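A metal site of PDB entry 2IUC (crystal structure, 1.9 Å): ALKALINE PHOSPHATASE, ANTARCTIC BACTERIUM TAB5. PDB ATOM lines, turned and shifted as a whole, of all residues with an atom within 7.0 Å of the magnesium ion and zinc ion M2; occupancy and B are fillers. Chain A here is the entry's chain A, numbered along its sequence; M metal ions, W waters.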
ATOM      1  N   ILE A  41     -12.596  26.831 -11.094  1.00  0.00           N
ATOM      2  CA  ILE A  41     -13.492  27.159 -12.207  1.00  0.00           C
ATOM      3  C   ILE A  41     -14.545  26.109 -12.166  1.00  0.00           C
ATOM      4  O   ILE A  41     -14.234  24.882 -12.213  1.00  0.00           O
ATOM      5  CB  ILE A  41     -12.715  27.102 -13.599  1.00  0.00           C
ATOM      6  CG1 ILE A  41     -11.579  28.123 -13.634  1.00  0.00           C
ATOM      7  CG2 ILE A  41     -13.745  27.173 -14.805  1.00  0.00           C
ATOM      8  CD1 ILE A  41     -10.689  28.028 -14.907  1.00  0.00           C
ATOM      9  N   SER A  42     -15.808  26.541 -12.029  1.00  0.00           N
ATOM     10  CA  SER A  42     -16.936  25.633 -12.071  1.00  0.00           C
ATOM     11  C   SER A  42     -17.446  25.794 -13.527  1.00  0.00           C
ATOM     12  O   SER A  42     -18.068  26.816 -13.894  1.00  0.00           O
ATOM     13  CB  SER A  42     -17.970  26.093 -11.080  1.00  0.00           C
ATOM     14  OG  SER A  42     -18.052  27.526 -11.158  1.00  0.00           O
ATOM     15  N   ASP A  43     -17.188  24.786 -14.334  1.00  0.00           N
ATOM     16  CA  ASP A  43     -17.620  24.846 -15.707  1.00  0.00           C
ATOM     17  C   ASP A  43     -19.101  24.850 -15.859  1.00  0.00           C
ATOM     18  O   ASP A  43     -19.772  23.908 -15.417  1.00  0.00           O
ATOM     19  CB  ASP A  43     -17.057  23.669 -16.498  1.00  0.00           C
ATOM     20  CG  ASP A  43     -17.053  23.946 -18.036  1.00  0.00           C
ATOM     21  OD1 ASP A  43     -18.072  24.275 -18.596  1.00  0.00           O
ATOM     22  OD2 ASP A  43     -15.996  23.847 -18.675  1.00  0.00           O
ATOM     23  N   GLY A  44     -19.637  25.900 -16.495  1.00  0.00           N
ATOM     24  CA  GLY A  44     -21.072  25.925 -16.753  1.00  0.00           C
ATOM     25  C   GLY A  44     -21.988  26.354 -15.624  1.00  0.00           C
ATOM     26  O   GLY A  44     -23.182  26.173 -15.739  1.00  0.00           O
ATOM     27  N   THR A  82     -20.121  31.937 -25.516  1.00  0.00           N
ATOM     28  CA  THR A  82     -18.798  31.380 -25.548  1.00  0.00           C
ATOM     29  C   THR A  82     -18.878  29.852 -25.396  1.00  0.00           C
ATOM     30  O   THR A  82     -19.884  29.333 -24.917  1.00  0.00           O
ATOM     31  CB  THR A  82     -17.956  31.939 -24.351  1.00  0.00           C
ATOM     32  OG1 THR A  82     -16.582  31.564 -24.548  1.00  0.00           O
ATOM     33  CG2 THR A  82     -18.433  31.304 -23.061  1.00  0.00           C
ATOM     34  N   ASP A  83     -17.835  29.159 -25.784  1.00  0.00           N
ATOM     35  CA  ASP A  83     -17.649  27.753 -25.322  1.00  0.00           C
ATOM     36  C   ASP A  83     -16.565  27.730 -24.243  1.00  0.00           C
ATOM     37  O   ASP A  83     -15.979  28.773 -23.891  1.00  0.00           O
ATOM     38  CB  ASP A  83     -17.339  26.795 -26.536  1.00  0.00           C
ATOM     39  CG  ASP A  83     -15.870  26.809 -26.980  1.00  0.00           C
ATOM     40  OD1 ASP A  83     -15.106  27.820 -26.852  1.00  0.00           O
ATOM     41  OD2 ASP A  83     -15.449  25.773 -27.523  1.00  0.00           O
ATOM     42  N   SER A  84     -16.244  26.542 -23.753  1.00  0.00           N
ATOM     43  CA  SER A  84     -15.255  26.459 -22.661  1.00  0.00           C
ATOM     44  C   SER A  84     -13.842  26.819 -23.092  1.00  0.00           C
ATOM     45  O   SER A  84     -12.965  27.209 -22.267  1.00  0.00           O
ATOM     46  CB  SER A  84     -15.172  25.003 -22.264  1.00  0.00           C
ATOM     47  OG  SER A  84     -16.402  24.682 -21.703  1.00  0.00           O
ATOM     48  N   ALA A  85     -13.559  26.576 -24.386  1.00  0.00           N
ATOM     49  CA  ALA A  85     -12.201  26.784 -24.908  1.00  0.00           C
ATOM     50  C   ALA A  85     -11.850  28.280 -24.890  1.00  0.00           C
ATOM     51  O   ALA A  85     -10.770  28.654 -24.312  1.00  0.00           O
ATOM     52  CB  ALA A  85     -12.074  26.235 -26.285  1.00  0.00           C
ATOM     53  N   GLY A  87     -13.513  30.610 -23.375  1.00  0.00           N
ATOM     54  CA  GLY A  87     -13.814  30.965 -21.978  1.00  0.00           C
ATOM     55  C   GLY A  87     -12.603  30.786 -21.084  1.00  0.00           C
ATOM     56  O   GLY A  87     -12.298  31.657 -20.343  1.00  0.00           O
ATOM     57  N   ALA A  88     -11.948  29.632 -21.141  1.00  0.00           N
ATOM     58  CA  ALA A  88     -10.835  29.399 -20.290  1.00  0.00           C
ATOM     59  C   ALA A  88      -9.577  30.128 -20.804  1.00  0.00           C
ATOM     60  O   ALA A  88      -8.690  30.420 -19.997  1.00  0.00           O
ATOM     61  CB  ALA A  88     -10.530  27.953 -20.228  1.00  0.00           C
ATOM     62  N   SER A 131     -12.855  16.195 -15.575  1.00  0.00           N
ATOM     63  CA  SER A 131     -12.922  15.696 -16.955  1.00  0.00           C
ATOM     64  C   SER A 131     -11.591  15.043 -17.285  1.00  0.00           C
ATOM     65  O   SER A 131     -10.682  14.909 -16.404  1.00  0.00           O
ATOM     66  CB  SER A 131     -13.167  16.890 -17.899  1.00  0.00           C
ATOM     67  OG  SER A 131     -12.068  17.781 -17.768  1.00  0.00           O
ATOM     68  N   HIS A 135      -9.272  18.017 -21.663  1.00  0.00           N
ATOM     69  CA  HIS A 135     -10.542  18.755 -21.947  1.00  0.00           C
ATOM     70  C   HIS A 135     -10.270  20.291 -22.004  1.00  0.00           C
ATOM     71  O   HIS A 135      -9.235  20.708 -21.567  1.00  0.00           O
ATOM     72  CB  HIS A 135     -11.657  18.436 -20.912  1.00  0.00           C
ATOM     73  CG  HIS A 135     -13.037  18.469 -21.511  1.00  0.00           C
ATOM     74  ND1 HIS A 135     -13.896  19.539 -21.339  1.00  0.00           N
ATOM     75  CD2 HIS A 135     -13.693  17.576 -22.318  1.00  0.00           C
ATOM     76  CE1 HIS A 135     -15.015  19.301 -22.020  1.00  0.00           C
ATOM     77  NE2 HIS A 135     -14.918  18.114 -22.611  1.00  0.00           N
ATOM     78  N   ALA A 136     -11.170  21.074 -22.579  1.00  0.00           N
ATOM     79  CA  ALA A 136     -10.823  22.420 -23.013  1.00  0.00           C
ATOM     80  C   ALA A 136     -10.331  23.320 -21.848  1.00  0.00           C
ATOM     81  O   ALA A 136      -9.474  24.191 -21.999  1.00  0.00           O
ATOM     82  CB  ALA A 136     -12.010  22.988 -23.638  1.00  0.00           C
ATOM     83  N   THR A 137     -10.914  23.139 -20.681  1.00  0.00           N
ATOM     84  CA  THR A 137     -10.592  24.071 -19.542  1.00  0.00           C
ATOM     85  C   THR A 137      -9.171  23.861 -19.054  1.00  0.00           C
ATOM     86  O   THR A 137      -8.370  24.797 -19.121  1.00  0.00           O
ATOM     87  CB  THR A 137     -11.682  24.012 -18.438  1.00  0.00           C
ATOM     88  OG1 THR A 137     -12.982  24.238 -19.018  1.00  0.00           O
ATOM     89  CG2 THR A 137     -11.413  24.992 -17.276  1.00  0.00           C
ATOM     90  N   PRO A 138      -8.825  22.599 -18.572  1.00  0.00           N
ATOM     91  CA  PRO A 138      -7.408  22.411 -18.187  1.00  0.00           C
ATOM     92  C   PRO A 138      -6.417  22.670 -19.320  1.00  0.00           C
ATOM     93  O   PRO A 138      -5.281  23.188 -19.113  1.00  0.00           O
ATOM     94  CB  PRO A 138      -7.360  20.924 -17.717  1.00  0.00           C
ATOM     95  CG  PRO A 138      -8.628  20.256 -18.188  1.00  0.00           C
ATOM     96  CD  PRO A 138      -9.634  21.363 -18.427  1.00  0.00           C
ATOM     97  N   ARG A 148      -9.982  22.760 -29.890  1.00  0.00           N
ATOM     98  CA  ARG A 148     -10.054  22.002 -28.646  1.00  0.00           C
ATOM     99  C   ARG A 148     -10.249  20.524 -28.897  1.00  0.00           C
ATOM    100  O   ARG A 148     -10.048  19.757 -27.988  1.00  0.00           O
ATOM    101  CB  ARG A 148     -11.309  22.444 -27.856  1.00  0.00           C
ATOM    102  CG  ARG A 148     -12.642  22.255 -28.653  1.00  0.00           C
ATOM    103  CD  ARG A 148     -13.702  22.852 -27.834  1.00  0.00           C
ATOM    104  NE  ARG A 148     -13.961  22.052 -26.622  1.00  0.00           N
ATOM    105  CZ  ARG A 148     -14.919  22.320 -25.726  1.00  0.00           C
ATOM    106  NH1 ARG A 148     -15.671  23.456 -25.873  1.00  0.00           N
ATOM    107  NH2 ARG A 148     -15.110  21.494 -24.678  1.00  0.00           N
ATOM    108  N   GLU A 254     -10.672  22.496 -11.521  1.00  0.00           N
ATOM    109  CA  GLU A 254     -11.913  22.678 -12.257  1.00  0.00           C
ATOM    110  C   GLU A 254     -12.951  21.649 -11.815  1.00  0.00           C
ATOM    111  O   GLU A 254     -12.661  20.413 -11.821  1.00  0.00           O
ATOM    112  CB  GLU A 254     -11.686  22.485 -13.776  1.00  0.00           C
ATOM    113  CG  GLU A 254     -13.009  22.882 -14.486  1.00  0.00           C
ATOM    114  CD  GLU A 254     -13.139  22.264 -15.878  1.00  0.00           C
ATOM    115  OE1 GLU A 254     -12.396  21.325 -16.206  1.00  0.00           O
ATOM    116  OE2 GLU A 254     -13.971  22.756 -16.636  1.00  0.00           O
ATOM    117  N   GLY A 255     -14.133  22.143 -11.428  1.00  0.00           N
ATOM    118  CA  GLY A 255     -15.398  21.332 -11.309  1.00  0.00           C
ATOM    119  C   GLY A 255     -16.004  21.159 -12.727  1.00  0.00           C
ATOM    120  O   GLY A 255     -16.873  21.945 -13.149  1.00  0.00           O
ATOM    121  N   SER A 256     -15.448  20.210 -13.484  1.00  0.00           N
ATOM    122  CA  SER A 256     -15.702  20.028 -14.946  1.00  0.00           C
ATOM    123  C   SER A 256     -17.078  19.572 -15.329  1.00  0.00           C
ATOM    124  O   SER A 256     -17.579  19.924 -16.443  1.00  0.00           O
ATOM    125  CB  SER A 256     -14.706  19.013 -15.550  1.00  0.00           C
ATOM    126  OG  SER A 256     -13.419  19.241 -15.054  1.00  0.00           O
ATOM    127  N   GLN A 257     -17.710  18.772 -14.465  1.00  0.00           N
ATOM    128  CA  GLN A 257     -18.904  18.018 -14.911  1.00  0.00           C
ATOM    129  C   GLN A 257     -20.190  18.753 -14.586  1.00  0.00           C
ATOM    130  O   GLN A 257     -21.299  18.354 -14.996  1.00  0.00           O
ATOM    131  CB  GLN A 257     -18.892  16.596 -14.320  1.00  0.00           C
ATOM    132  CG  GLN A 257     -17.645  15.860 -14.829  1.00  0.00           C
ATOM    133  CD  GLN A 257     -17.746  14.364 -14.529  1.00  0.00           C
ATOM    134  OE1 GLN A 257     -18.829  13.822 -14.529  1.00  0.00           O
ATOM    135  NE2 GLN A 257     -16.599  13.692 -14.338  1.00  0.00           N
ATOM    136  N   ASP A 259     -21.116  21.418 -15.999  1.00  0.00           N
ATOM    137  CA  ASP A 259     -21.607  21.774 -17.354  1.00  0.00           C
ATOM    138  C   ASP A 259     -22.269  20.547 -18.020  1.00  0.00           C
ATOM    139  O   ASP A 259     -23.219  20.634 -18.811  1.00  0.00           O
ATOM    140  CB  ASP A 259     -20.366  22.180 -18.127  1.00  0.00           C
ATOM    141  CG  ASP A 259     -20.642  22.328 -19.634  1.00  0.00           C
ATOM    142  OD1 ASP A 259     -21.193  23.368 -20.015  1.00  0.00           O
ATOM    143  OD2 ASP A 259     -20.264  21.415 -20.405  1.00  0.00           O
ATOM    144  N   TRP A 260     -21.767  19.361 -17.712  1.00  0.00           N
ATOM    145  CA  TRP A 260     -22.316  18.182 -18.434  1.00  0.00           C
ATOM    146  C   TRP A 260     -23.689  17.871 -17.943  1.00  0.00           C
ATOM    147  O   TRP A 260     -24.523  17.415 -18.707  1.00  0.00           O
ATOM    148  CB  TRP A 260     -21.375  16.960 -18.338  1.00  0.00           C
ATOM    149  CG  TRP A 260     -19.923  17.240 -18.832  1.00  0.00           C
ATOM    150  CD1 TRP A 260     -19.450  18.390 -19.482  1.00  0.00           C
ATOM    151  CD2 TRP A 260     -18.804  16.354 -18.732  1.00  0.00           C
ATOM    152  NE1 TRP A 260     -18.117  18.247 -19.776  1.00  0.00           N
ATOM    153  CE2 TRP A 260     -17.690  16.992 -19.341  1.00  0.00           C
ATOM    154  CE3 TRP A 260     -18.641  15.044 -18.227  1.00  0.00           C
ATOM    155  CZ2 TRP A 260     -16.430  16.394 -19.407  1.00  0.00           C
ATOM    156  CZ3 TRP A 260     -17.398  14.440 -18.276  1.00  0.00           C
ATOM    157  CH2 TRP A 260     -16.316  15.087 -18.889  1.00  0.00           C
ATOM    158  N   HIS A 263     -25.947  20.402 -19.813  1.00  0.00           N
ATOM    159  CA  HIS A 263     -26.199  19.961 -21.200  1.00  0.00           C
ATOM    160  C   HIS A 263     -27.178  18.815 -21.206  1.00  0.00           C
ATOM    161  O   HIS A 263     -27.958  18.719 -22.133  1.00  0.00           O
ATOM    162  CB  HIS A 263     -24.923  19.444 -21.889  1.00  0.00           C
ATOM    163  CG  HIS A 263     -24.012  20.526 -22.396  1.00  0.00           C
ATOM    164  ND1 HIS A 263     -24.418  21.499 -23.306  1.00  0.00           N
ATOM    165  CD2 HIS A 263     -22.692  20.750 -22.167  1.00  0.00           C
ATOM    166  CE1 HIS A 263     -23.394  22.292 -23.589  1.00  0.00           C
ATOM    167  NE2 HIS A 263     -22.333  21.849 -22.921  1.00  0.00           N
ATOM    168  N   ASP A 301     -16.714  29.597 -16.474  1.00  0.00           N
ATOM    169  CA  ASP A 301     -16.547  30.092 -17.841  1.00  0.00           C
ATOM    170  C   ASP A 301     -17.800  30.674 -18.527  1.00  0.00           C
ATOM    171  O   ASP A 301     -17.673  31.549 -19.399  1.00  0.00           O
ATOM    172  CB  ASP A 301     -15.868  29.043 -18.734  1.00  0.00           C
ATOM    173  CG  ASP A 301     -16.576  27.648 -18.713  1.00  0.00           C
ATOM    174  OD1 ASP A 301     -17.572  27.387 -17.987  1.00  0.00           O
ATOM    175  OD2 ASP A 301     -16.205  26.814 -19.570  1.00  0.00           O
ATOM    176  N   HIS A 302     -18.996  30.177 -18.184  1.00  0.00           N
ATOM    177  CA  HIS A 302     -20.280  30.583 -18.788  1.00  0.00           C
ATOM    178  C   HIS A 302     -21.298  29.698 -18.028  1.00  0.00           C
ATOM    179  O   HIS A 302     -20.912  28.822 -17.215  1.00  0.00           O
ATOM    180  CB  HIS A 302     -20.308  30.235 -20.331  1.00  0.00           C
ATOM    181  CG  HIS A 302     -20.020  28.768 -20.561  1.00  0.00           C
ATOM    182  ND1 HIS A 302     -20.941  27.790 -20.275  1.00  0.00           N
ATOM    183  CD2 HIS A 302     -18.882  28.117 -20.879  1.00  0.00           C
ATOM    184  CE1 HIS A 302     -20.393  26.611 -20.381  1.00  0.00           C
ATOM    185  NE2 HIS A 302     -19.161  26.770 -20.778  1.00  0.00           N
ATOM    186  N   THR A 304     -24.685  27.038 -18.260  1.00  0.00           N
ATOM    187  CA  THR A 304     -25.286  26.040 -19.182  1.00  0.00           C
ATOM    188  C   THR A 304     -26.694  25.517 -18.813  1.00  0.00           C
ATOM    189  O   THR A 304     -26.981  25.120 -17.646  1.00  0.00           O
ATOM    190  CB  THR A 304     -24.419  24.775 -19.235  1.00  0.00           C
ATOM    191  OG1 THR A 304     -23.092  25.133 -19.521  1.00  0.00           O
ATOM    192  CG2 THR A 304     -24.949  23.760 -20.399  1.00  0.00           C
ATOM    193  N   HIS A 337     -25.045  26.464 -23.926  1.00  0.00           N
ATOM    194  CA  HIS A 337     -24.482  27.513 -23.041  1.00  0.00           C
ATOM    195  C   HIS A 337     -25.388  28.729 -23.124  1.00  0.00           C
ATOM    196  O   HIS A 337     -26.251  28.828 -24.018  1.00  0.00           O
ATOM    197  CB  HIS A 337     -23.051  27.860 -23.516  1.00  0.00           C
ATOM    198  CG  HIS A 337     -22.073  26.724 -23.379  1.00  0.00           C
ATOM    199  ND1 HIS A 337     -20.787  26.796 -23.863  1.00  0.00           N
ATOM    200  CD2 HIS A 337     -22.219  25.453 -22.873  1.00  0.00           C
ATOM    201  CE1 HIS A 337     -20.164  25.627 -23.648  1.00  0.00           C
ATOM    202  NE2 HIS A 337     -20.994  24.839 -22.989  1.00  0.00           N
HETATM  203 MG    MG M   1     -14.473  22.454 -18.726  1.00  0.00          MG
HETATM  204 ZN    ZN M   2     -17.608  25.407 -20.253  1.00  0.00          ZN
HETATM  205 ZN    ZN M   3     -20.659  22.956 -22.238  1.00  0.00          ZN
HETATM  206  O   HOH W   1     -13.008  20.790 -18.888  1.00  0.00           O
HETATM  207  O   HOH W   2     -14.568  22.284 -20.916  1.00  0.00           O
HETATM  208  O   HOH W   3     -16.027  21.060 -18.454  1.00  0.00           O
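The backbone NH of Asp 259 sits at hydrogen-bond distance from the backbone carbonyl oxygen of Asp 43 (2.9 Å). O of Gly 255 sits at hydrogen-bond distance from N of Asp 43, at 3.1 Å. OD1 of Asp 301 is in hydrogen-bond range of N of Gly 44 (2.9 Å). A ring nitrogen (NE2) of His 302 lies close to a ring nitrogen (ND1) of His 337, at 3.5 Å. N of Gly 44 lies close to O of His 302, 3.3 Å away. The side-chain carboxylate of Glu 254 lies within hydrogen-bond range of the side-chain hydroxyl of Ser 256 (2.6 Å).
Merely in contact with the magnesium ion: His 135. Four residues have an atom within 4 Å of the magnesium ion: Asp 43, His 135, Thr 137 and Glu 254. The nearest printed residue that does not touch the magnesium ion is Ser 84 (4.2 Å).
Of the 27 residues printed, 4 come within 4 Å of zinc ion M2.
The magnesium ion is bound by OD2 of Asp 43, water W3, OE2 of Glu 254, water W2, water W1 and OG1 of Thr 137.
Zinc ion M2 is bound by the side-chain hydroxyl (OG) of Ser 84 (2.0 Å), the side-chain carboxylate (OD1) of Asp 43 (2.1 Å), the side-chain carboxylate (OD2) of Asp 301 (2.1 Å) and a ring nitrogen (NE2) of His 302 (2.1 Å). Zinc ion M2 has four donor atoms within binding distance. Slightly farther from zinc ion M2 lies OD2 of Asp 43 (2.7 Å).
Water W1 lies within hydrogen-bond range of OE1 of Glu 254 (2.8 Å), ND1 of His 135 (2.9 Å) and OG of Ser 131 (3.3 Å).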
